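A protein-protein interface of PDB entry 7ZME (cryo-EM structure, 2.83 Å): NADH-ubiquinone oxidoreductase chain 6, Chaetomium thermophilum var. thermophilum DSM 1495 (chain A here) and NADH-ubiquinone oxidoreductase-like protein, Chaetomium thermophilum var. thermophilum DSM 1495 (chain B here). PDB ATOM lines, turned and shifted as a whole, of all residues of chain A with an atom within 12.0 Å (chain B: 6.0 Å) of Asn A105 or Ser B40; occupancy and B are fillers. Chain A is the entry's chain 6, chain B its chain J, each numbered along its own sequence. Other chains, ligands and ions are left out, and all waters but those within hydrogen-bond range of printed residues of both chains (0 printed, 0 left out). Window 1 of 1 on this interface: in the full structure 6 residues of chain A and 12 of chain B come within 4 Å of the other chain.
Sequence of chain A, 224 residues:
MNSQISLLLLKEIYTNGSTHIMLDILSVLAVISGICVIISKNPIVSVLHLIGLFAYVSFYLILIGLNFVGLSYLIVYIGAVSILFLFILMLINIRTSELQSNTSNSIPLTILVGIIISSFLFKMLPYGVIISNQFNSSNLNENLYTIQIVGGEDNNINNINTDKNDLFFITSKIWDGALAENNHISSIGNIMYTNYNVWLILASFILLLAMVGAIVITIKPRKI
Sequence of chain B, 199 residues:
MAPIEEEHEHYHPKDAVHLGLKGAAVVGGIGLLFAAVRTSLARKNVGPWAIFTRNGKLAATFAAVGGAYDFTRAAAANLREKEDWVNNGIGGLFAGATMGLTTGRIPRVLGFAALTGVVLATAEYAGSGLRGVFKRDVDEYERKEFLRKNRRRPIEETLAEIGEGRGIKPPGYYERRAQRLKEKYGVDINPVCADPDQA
Of chain A, only Asn A105 (3.6 Å) and Leu A109 (3.3 Å) come within 4 Å of Ser B40. Val B37 touches one residue of chain A. Of the printed residues of chain A, Ala B42 touches Asn A105. Of the printed residues of chain A, Asn B45 touches Asn A105 (3.4 Å). Of the printed residues of chain A, Pro B48 touches Ser A104, Ile A107 and Pro A108. Of the printed residues of chain A, Lys B44 touches Asn A105 (3.6 Å). Printed residues of chain B within 4 Å of Leu A109: Ala B36 (3.9 Å), Val B37 (3.7 Å) and Ser B40 (3.3 Å). Printed residues of chain B within 4 Å of Leu A112: Ala B36 (3.7 Å). Of the printed residues of chain B, Ile A107 touches Pro B48. Ser A106 touches none of the printed residues of chain B. The nearest printed residue of chain A that does not touch Lys B44 is Thr A103 (6.2 Å).
The backbone carbonyl oxygen of Ala B35 is in hydrogen-bond range of the side-chain hydroxyl of Thr B39 (2.6 Å). OG of Ser B40 is in hydrogen-bond range of O of Val B37 (2.9 Å).
Hydrophobic or aromatic side chains of chain B within 4 Å of the printed part of chain A: Ala B36, Val B37 and Pro B48. Hydrophobic or aromatic side chains of chain A that line the printed part of chain B: Ile A107, Pro A108, Leu A109 and Leu A112.
Ser A104 touches Pro B48 (O to CG, 3.5 Å). Asn A105 touches Thr B39. Asn A105 touches Ser B40. ND2 of Asn A105 touches O of Ala B42 (3.9 Å). Asn A105 touches Asn B45 (ND2 to CA, 3.4 Å). Ile A107 touches Pro B48. C of Pro A108 touches CB of Ala B36, at 3.99 Å. Pro A108 touches Pro B48. N of Leu A109 touches CB of Ala B36, at 3.9 Å. Leu A109 touches Val B37.
The backbone NH of Gly B47 lies within hydrogen-bond range of the side-chain amide oxygen of Asn A105, 3.3 Å away. The side-chain amide oxygen (OD1) of Asn A105 sits at hydrogen-bond distance from the backbone NH (N) of Val B46, 3.5 Å away.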
ATOM      1  N   SER A 101     -11.734  15.429 -21.853  1.00  0.00           N
ATOM      2  CA  SER A 101     -11.607  14.635 -20.605  1.00  0.00           C
ATOM      3  C   SER A 101     -11.311  13.163 -20.884  1.00  0.00           C
ATOM      4  O   SER A 101     -10.795  12.863 -21.978  1.00  0.00           O
ATOM      5  CB  SER A 101     -12.838  14.785 -19.748  1.00  0.00           C
ATOM      6  N   ASN A 102     -11.641  12.289 -19.933  1.00  0.00           N
ATOM      7  CA  ASN A 102     -11.487  10.853 -20.104  1.00  0.00           C
ATOM      8  C   ASN A 102     -12.528  10.124 -19.267  1.00  0.00           C
ATOM      9  O   ASN A 102     -12.780  10.492 -18.114  1.00  0.00           O
ATOM     10  CB  ASN A 102     -10.079  10.398 -19.704  1.00  0.00           C
ATOM     11  CG  ASN A 102      -9.698  10.844 -18.307  1.00  0.00           C
ATOM     12  OD1 ASN A 102      -9.623  12.040 -18.023  1.00  0.00           O
ATOM     13  ND2 ASN A 102      -9.457   9.883 -17.422  1.00  0.00           N
ATOM     14  N   THR A 103     -13.132   9.095 -19.851  1.00  0.00           N
ATOM     15  CA  THR A 103     -14.142   8.315 -19.156  1.00  0.00           C
ATOM     16  C   THR A 103     -13.488   7.281 -18.241  1.00  0.00           C
ATOM     17  O   THR A 103     -12.284   7.025 -18.301  1.00  0.00           O
ATOM     18  CB  THR A 103     -15.072   7.627 -20.154  1.00  0.00           C
ATOM     19  N   SER A 104     -14.310   6.682 -17.378  1.00  0.00           N
ATOM     20  CA  SER A 104     -13.864   5.647 -16.455  1.00  0.00           C
ATOM     21  C   SER A 104     -14.238   4.248 -16.934  1.00  0.00           C
ATOM     22  O   SER A 104     -14.101   3.280 -16.181  1.00  0.00           O
ATOM     23  CB  SER A 104     -14.433   5.900 -15.059  1.00  0.00           C
ATOM     24  N   ASN A 105     -14.704   4.125 -18.173  1.00  0.00           N
ATOM     25  CA  ASN A 105     -15.096   2.844 -18.743  1.00  0.00           C
ATOM     26  C   ASN A 105     -13.906   1.957 -19.074  1.00  0.00           C
ATOM     27  O   ASN A 105     -14.100   0.788 -19.417  1.00  0.00           O
ATOM     28  CB  ASN A 105     -15.936   3.066 -20.003  1.00  0.00           C
ATOM     29  CG  ASN A 105     -17.131   3.961 -19.753  1.00  0.00           C
ATOM     30  OD1 ASN A 105     -17.514   4.197 -18.607  1.00  0.00           O
ATOM     31  ND2 ASN A 105     -17.723   4.472 -20.826  1.00  0.00           N
ATOM     32  N   SER A 106     -12.688   2.485 -18.985  1.00  0.00           N
ATOM     33  CA  SER A 106     -11.480   1.740 -19.301  1.00  0.00           C
ATOM     34  C   SER A 106     -10.913   0.978 -18.114  1.00  0.00           C
ATOM     35  O   SER A 106      -9.984   0.186 -18.296  1.00  0.00           O
ATOM     36  CB  SER A 106     -10.408   2.692 -19.835  1.00  0.00           C
ATOM     37  OG  SER A 106     -10.919   3.518 -20.868  1.00  0.00           O
ATOM     38  N   ILE A 107     -11.433   1.202 -16.912  1.00  0.00           N
ATOM     39  CA  ILE A 107     -10.925   0.556 -15.706  1.00  0.00           C
ATOM     40  C   ILE A 107     -11.105  -0.959 -15.770  1.00  0.00           C
ATOM     41  O   ILE A 107     -10.151  -1.687 -15.464  1.00  0.00           O
ATOM     42  CB  ILE A 107     -11.581   1.146 -14.447  1.00  0.00           C
ATOM     43  CG1 ILE A 107     -11.167   2.607 -14.273  1.00  0.00           C
ATOM     44  CG2 ILE A 107     -11.209   0.334 -13.216  1.00  0.00           C
ATOM     45  CD1 ILE A 107     -12.149   3.427 -13.479  1.00  0.00           C
ATOM     46  N   PRO A 108     -12.283  -1.494 -16.137  1.00  0.00           N
ATOM     47  CA  PRO A 108     -12.392  -2.961 -16.226  1.00  0.00           C
ATOM     48  C   PRO A 108     -11.406  -3.577 -17.196  1.00  0.00           C
ATOM     49  O   PRO A 108     -10.852  -4.647 -16.922  1.00  0.00           O
ATOM     50  CB  PRO A 108     -13.842  -3.176 -16.678  1.00  0.00           C
ATOM     51  CG  PRO A 108     -14.558  -1.970 -16.214  1.00  0.00           C
ATOM     52  CD  PRO A 108     -13.585  -0.848 -16.386  1.00  0.00           C
ATOM     53  N   LEU A 109     -11.170  -2.924 -18.332  1.00  0.00           N
ATOM     54  CA  LEU A 109     -10.185  -3.421 -19.281  1.00  0.00           C
ATOM     55  C   LEU A 109      -8.773  -3.264 -18.732  1.00  0.00           C
ATOM     56  O   LEU A 109      -7.916  -4.123 -18.960  1.00  0.00           O
ATOM     57  CB  LEU A 109     -10.354  -2.698 -20.619  1.00  0.00           C
ATOM     58  CG  LEU A 109      -9.572  -3.135 -21.856  1.00  0.00           C
ATOM     59  CD1 LEU A 109     -10.362  -2.753 -23.082  1.00  0.00           C
ATOM     60  CD2 LEU A 109      -8.201  -2.491 -21.915  1.00  0.00           C
ATOM     61  N   THR A 110      -8.519  -2.171 -18.005  1.00  0.00           N
ATOM     62  CA  THR A 110      -7.207  -1.955 -17.401  1.00  0.00           C
ATOM     63  C   THR A 110      -6.857  -3.059 -16.414  1.00  0.00           C
ATOM     64  O   THR A 110      -5.735  -3.578 -16.425  1.00  0.00           O
ATOM     65  CB  THR A 110      -7.176  -0.594 -16.705  1.00  0.00           C
ATOM     66  OG1 THR A 110      -7.463   0.441 -17.655  1.00  0.00           O
ATOM     67  CG2 THR A 110      -5.825  -0.346 -16.051  1.00  0.00           C
ATOM     68  N   ILE A 111      -7.802  -3.430 -15.551  1.00  0.00           N
ATOM     69  CA  ILE A 111      -7.547  -4.485 -14.574  1.00  0.00           C
ATOM     70  C   ILE A 111      -7.297  -5.811 -15.279  1.00  0.00           C
ATOM     71  O   ILE A 111      -6.355  -6.541 -14.953  1.00  0.00           O
ATOM     72  CB  ILE A 111      -8.716  -4.586 -13.578  1.00  0.00           C
ATOM     73  CG1 ILE A 111      -8.800  -3.319 -12.724  1.00  0.00           C
ATOM     74  CG2 ILE A 111      -8.562  -5.815 -12.695  1.00  0.00           C
ATOM     75  CD1 ILE A 111      -7.620  -3.128 -11.800  1.00  0.00           C
ATOM     76  N   LEU A 112      -8.139  -6.140 -16.260  1.00  0.00           N
ATOM     77  CA  LEU A 112      -8.001  -7.410 -16.965  1.00  0.00           C
ATOM     78  C   LEU A 112      -6.714  -7.456 -17.777  1.00  0.00           C
ATOM     79  O   LEU A 112      -5.937  -8.412 -17.673  1.00  0.00           O
ATOM     80  CB  LEU A 112      -9.211  -7.637 -17.869  1.00  0.00           C
ATOM     81  CG  LEU A 112     -10.463  -8.209 -17.203  1.00  0.00           C
ATOM     82  CD1 LEU A 112     -11.528  -8.485 -18.248  1.00  0.00           C
ATOM     83  CD2 LEU A 112     -10.127  -9.468 -16.419  1.00  0.00           C
ATOM     84  N   VAL A 113      -6.471  -6.430 -18.595  1.00  0.00           N
ATOM     85  CA  VAL A 113      -5.277  -6.416 -19.436  1.00  0.00           C
ATOM     86  C   VAL A 113      -4.024  -6.340 -18.578  1.00  0.00           C
ATOM     87  O   VAL A 113      -3.011  -6.988 -18.871  1.00  0.00           O
ATOM     88  CB  VAL A 113      -5.352  -5.256 -20.447  1.00  0.00           C
ATOM     89  CG1 VAL A 113      -3.989  -4.980 -21.058  1.00  0.00           C
ATOM     90  CG2 VAL A 113      -6.364  -5.575 -21.532  1.00  0.00           C
ATOM     91  N   GLY A 114      -4.072  -5.560 -17.497  1.00  0.00           N
ATOM     92  CA  GLY A 114      -2.908  -5.446 -16.634  1.00  0.00           C
ATOM     93  C   GLY A 114      -2.525  -6.764 -15.993  1.00  0.00           C
ATOM     94  O   GLY A 114      -1.355  -7.151 -15.991  1.00  0.00           O
ATOM     95  N   ALA B  35     -16.468  -8.551 -22.701  1.00  0.00           N
ATOM     96  CA  ALA B  35     -17.367  -7.640 -22.006  1.00  0.00           C
ATOM     97  C   ALA B  35     -16.641  -6.367 -21.586  1.00  0.00           C
ATOM     98  O   ALA B  35     -17.181  -5.265 -21.725  1.00  0.00           O
ATOM     99  CB  ALA B  35     -17.987  -8.338 -20.796  1.00  0.00           C
ATOM    100  N   ALA B  36     -15.417  -6.500 -21.071  1.00  0.00           N
ATOM    101  CA  ALA B  36     -14.649  -5.323 -20.674  1.00  0.00           C
ATOM    102  C   ALA B  36     -14.240  -4.490 -21.876  1.00  0.00           C
ATOM    103  O   ALA B  36     -14.157  -3.263 -21.780  1.00  0.00           O
ATOM    104  CB  ALA B  36     -13.416  -5.742 -19.877  1.00  0.00           C
ATOM    105  N   VAL B  37     -13.972  -5.138 -23.009  1.00  0.00           N
ATOM    106  CA  VAL B  37     -13.603  -4.412 -24.216  1.00  0.00           C
ATOM    107  C   VAL B  37     -14.804  -3.677 -24.788  1.00  0.00           C
ATOM    108  O   VAL B  37     -14.687  -2.540 -25.259  1.00  0.00           O
ATOM    109  CB  VAL B  37     -12.979  -5.384 -25.229  1.00  0.00           C
ATOM    110  CG1 VAL B  37     -12.922  -4.764 -26.615  1.00  0.00           C
ATOM    111  CG2 VAL B  37     -11.603  -5.785 -24.757  1.00  0.00           C
ATOM    112  N   ARG B  38     -15.978  -4.308 -24.759  1.00  0.00           N
ATOM    113  CA  ARG B  38     -17.187  -3.640 -25.227  1.00  0.00           C
ATOM    114  C   ARG B  38     -17.543  -2.469 -24.322  1.00  0.00           C
ATOM    115  O   ARG B  38     -18.079  -1.457 -24.783  1.00  0.00           O
ATOM    116  CB  ARG B  38     -18.334  -4.646 -25.309  1.00  0.00           C
ATOM    117  CG  ARG B  38     -19.632  -4.088 -25.861  1.00  0.00           C
ATOM    118  CD  ARG B  38     -20.692  -5.174 -25.957  1.00  0.00           C
ATOM    119  NE  ARG B  38     -21.944  -4.677 -26.522  1.00  0.00           N
ATOM    120  CZ  ARG B  38     -22.934  -4.162 -25.801  1.00  0.00           C
ATOM    121  NH1 ARG B  38     -22.823  -4.076 -24.483  1.00  0.00           N
ATOM    122  NH2 ARG B  38     -24.038  -3.734 -26.398  1.00  0.00           N
ATOM    123  N   THR B  39     -17.240  -2.589 -23.028  1.00  0.00           N
ATOM    124  CA  THR B  39     -17.449  -1.481 -22.106  1.00  0.00           C
ATOM    125  C   THR B  39     -16.548  -0.299 -22.439  1.00  0.00           C
ATOM    126  O   THR B  39     -16.990   0.854 -22.407  1.00  0.00           O
ATOM    127  CB  THR B  39     -17.198  -1.947 -20.673  1.00  0.00           C
ATOM    128  OG1 THR B  39     -17.949  -3.139 -20.417  1.00  0.00           O
ATOM    129  CG2 THR B  39     -17.599  -0.868 -19.679  1.00  0.00           C
ATOM    130  N   SER B  40     -15.286  -0.568 -22.781  1.00  0.00           N
ATOM    131  CA  SER B  40     -14.318   0.531 -23.042  1.00  0.00           C
ATOM    132  C   SER B  40     -14.610   1.228 -24.365  1.00  0.00           C
ATOM    133  O   SER B  40     -14.144   2.361 -24.545  1.00  0.00           O
ATOM    134  CB  SER B  40     -12.917   0.023 -23.034  1.00  0.00           C
ATOM    135  OG  SER B  40     -12.661  -0.740 -24.200  1.00  0.00           O
ATOM    136  N   LEU B  41     -15.355   0.578 -25.246  1.00  0.00           N
ATOM    137  CA  LEU B  41     -15.590   1.146 -26.594  1.00  0.00           C
ATOM    138  C   LEU B  41     -16.951   1.843 -26.595  1.00  0.00           C
ATOM    139  O   LEU B  41     -17.402   2.254 -27.675  1.00  0.00           O
ATOM    140  CB  LEU B  41     -15.506   0.009 -27.615  1.00  0.00           C
ATOM    141  CG  LEU B  41     -14.099  -0.483 -27.931  1.00  0.00           C
ATOM    142  CD1 LEU B  41     -14.139  -1.559 -29.003  1.00  0.00           C
ATOM    143  CD2 LEU B  41     -13.221   0.675 -28.372  1.00  0.00           C
ATOM    144  N   ALA B  42     -17.570   1.956 -25.422  1.00  0.00           N
ATOM    145  CA  ALA B  42     -18.880   2.633 -25.282  1.00  0.00           C
ATOM    146  C   ALA B  42     -18.678   4.146 -25.395  1.00  0.00           C
ATOM    147  O   ALA B  42     -17.815   4.674 -24.670  1.00  0.00           O
ATOM    148  CB  ALA B  42     -19.502   2.260 -23.964  1.00  0.00           C
ATOM    149  N   ARG B  43     -19.445   4.814 -26.263  1.00  0.00           N
ATOM    150  CA  ARG B  43     -19.252   6.246 -26.468  1.00  0.00           C
ATOM    151  C   ARG B  43     -19.739   7.054 -25.271  1.00  0.00           C
ATOM    152  O   ARG B  43     -19.085   8.020 -24.862  1.00  0.00           O
ATOM    153  CB  ARG B  43     -19.961   6.691 -27.746  1.00  0.00           C
ATOM    154  CG  ARG B  43     -19.345   6.132 -29.019  1.00  0.00           C
ATOM    155  CD  ARG B  43     -20.182   6.475 -30.239  1.00  0.00           C
ATOM    156  NE  ARG B  43     -19.466   6.208 -31.484  1.00  0.00           N
ATOM    157  CZ  ARG B  43     -19.569   5.081 -32.179  1.00  0.00           C
ATOM    158  NH1 ARG B  43     -18.879   4.927 -33.300  1.00  0.00           N
ATOM    159  NH2 ARG B  43     -20.361   4.106 -31.754  1.00  0.00           N
ATOM    160  N   LYS B  44     -20.877   6.678 -24.698  1.00  0.00           N
ATOM    161  CA  LYS B  44     -21.434   7.376 -23.546  1.00  0.00           C
ATOM    162  C   LYS B  44     -20.866   6.768 -22.269  1.00  0.00           C
ATOM    163  O   LYS B  44     -20.925   5.549 -22.078  1.00  0.00           O
ATOM    164  CB  LYS B  44     -22.959   7.291 -23.548  1.00  0.00           C
ATOM    165  CG  LYS B  44     -23.612   7.797 -24.822  1.00  0.00           C
ATOM    166  CD  LYS B  44     -23.324   9.272 -25.045  1.00  0.00           C
ATOM    167  CE  LYS B  44     -23.968   9.771 -26.328  1.00  0.00           C
ATOM    168  NZ  LYS B  44     -23.685  11.213 -26.567  1.00  0.00           N
ATOM    169  N   ASN B  45     -20.311   7.614 -21.403  1.00  0.00           N
ATOM    170  CA  ASN B  45     -19.797   7.133 -20.129  1.00  0.00           C
ATOM    171  C   ASN B  45     -20.939   6.622 -19.260  1.00  0.00           C
ATOM    172  O   ASN B  45     -21.973   7.277 -19.113  1.00  0.00           O
ATOM    173  CB  ASN B  45     -19.030   8.244 -19.409  1.00  0.00           C
ATOM    174  CG  ASN B  45     -19.901   9.441 -19.088  1.00  0.00           C
ATOM    175  OD1 ASN B  45     -20.761   9.828 -19.878  1.00  0.00           O
ATOM    176  ND2 ASN B  45     -19.681  10.037 -17.921  1.00  0.00           N
ATOM    177  N   VAL B  46     -20.749   5.434 -18.691  1.00  0.00           N
ATOM    178  CA  VAL B  46     -21.800   4.763 -17.935  1.00  0.00           C
ATOM    179  C   VAL B  46     -21.273   4.293 -16.586  1.00  0.00           C
ATOM    180  O   VAL B  46     -22.049   3.895 -15.710  1.00  0.00           O
ATOM    181  CB  VAL B  46     -22.389   3.590 -18.740  1.00  0.00           C
ATOM    182  CG1 VAL B  46     -23.064   4.097 -20.002  1.00  0.00           C
ATOM    183  CG2 VAL B  46     -21.288   2.620 -19.112  1.00  0.00           C
ATOM    184  N   GLY B  47     -19.956   4.336 -16.406  1.00  0.00           N
ATOM    185  CA  GLY B  47     -19.353   3.977 -15.145  1.00  0.00           C
ATOM    186  C   GLY B  47     -18.585   2.671 -15.195  1.00  0.00           C
ATOM    187  O   GLY B  47     -18.861   1.788 -16.012  1.00  0.00           O
ATOM    188  N   PRO B  48     -17.589   2.535 -14.314  1.00  0.00           N
ATOM    189  CA  PRO B  48     -16.779   1.303 -14.308  1.00  0.00           C
ATOM    190  C   PRO B  48     -17.576   0.045 -14.011  1.00  0.00           C
ATOM    191  O   PRO B  48     -17.280  -1.016 -14.577  1.00  0.00           O
ATOM    192  CB  PRO B  48     -15.733   1.579 -13.216  1.00  0.00           C
ATOM    193  CG  PRO B  48     -15.731   3.068 -13.042  1.00  0.00           C
ATOM    194  CD  PRO B  48     -17.134   3.503 -13.304  1.00  0.00           C
ATOM    195  N   ASN B  55     -22.974  -5.370 -19.882  1.00  0.00           N
ATOM    196  CA  ASN B  55     -22.048  -6.348 -20.435  1.00  0.00           C
ATOM    197  C   ASN B  55     -22.092  -7.682 -19.704  1.00  0.00           C
ATOM    198  O   ASN B  55     -21.420  -8.625 -20.134  1.00  0.00           O
ATOM    199  CB  ASN B  55     -20.622  -5.794 -20.407  1.00  0.00           C
ATOM    200  CG  ASN B  55     -20.387  -4.749 -21.471  1.00  0.00           C
ATOM    201  OD1 ASN B  55     -20.027  -3.611 -21.172  1.00  0.00           O
ATOM    202  ND2 ASN B  55     -20.584  -5.130 -22.724  1.00  0.00           N
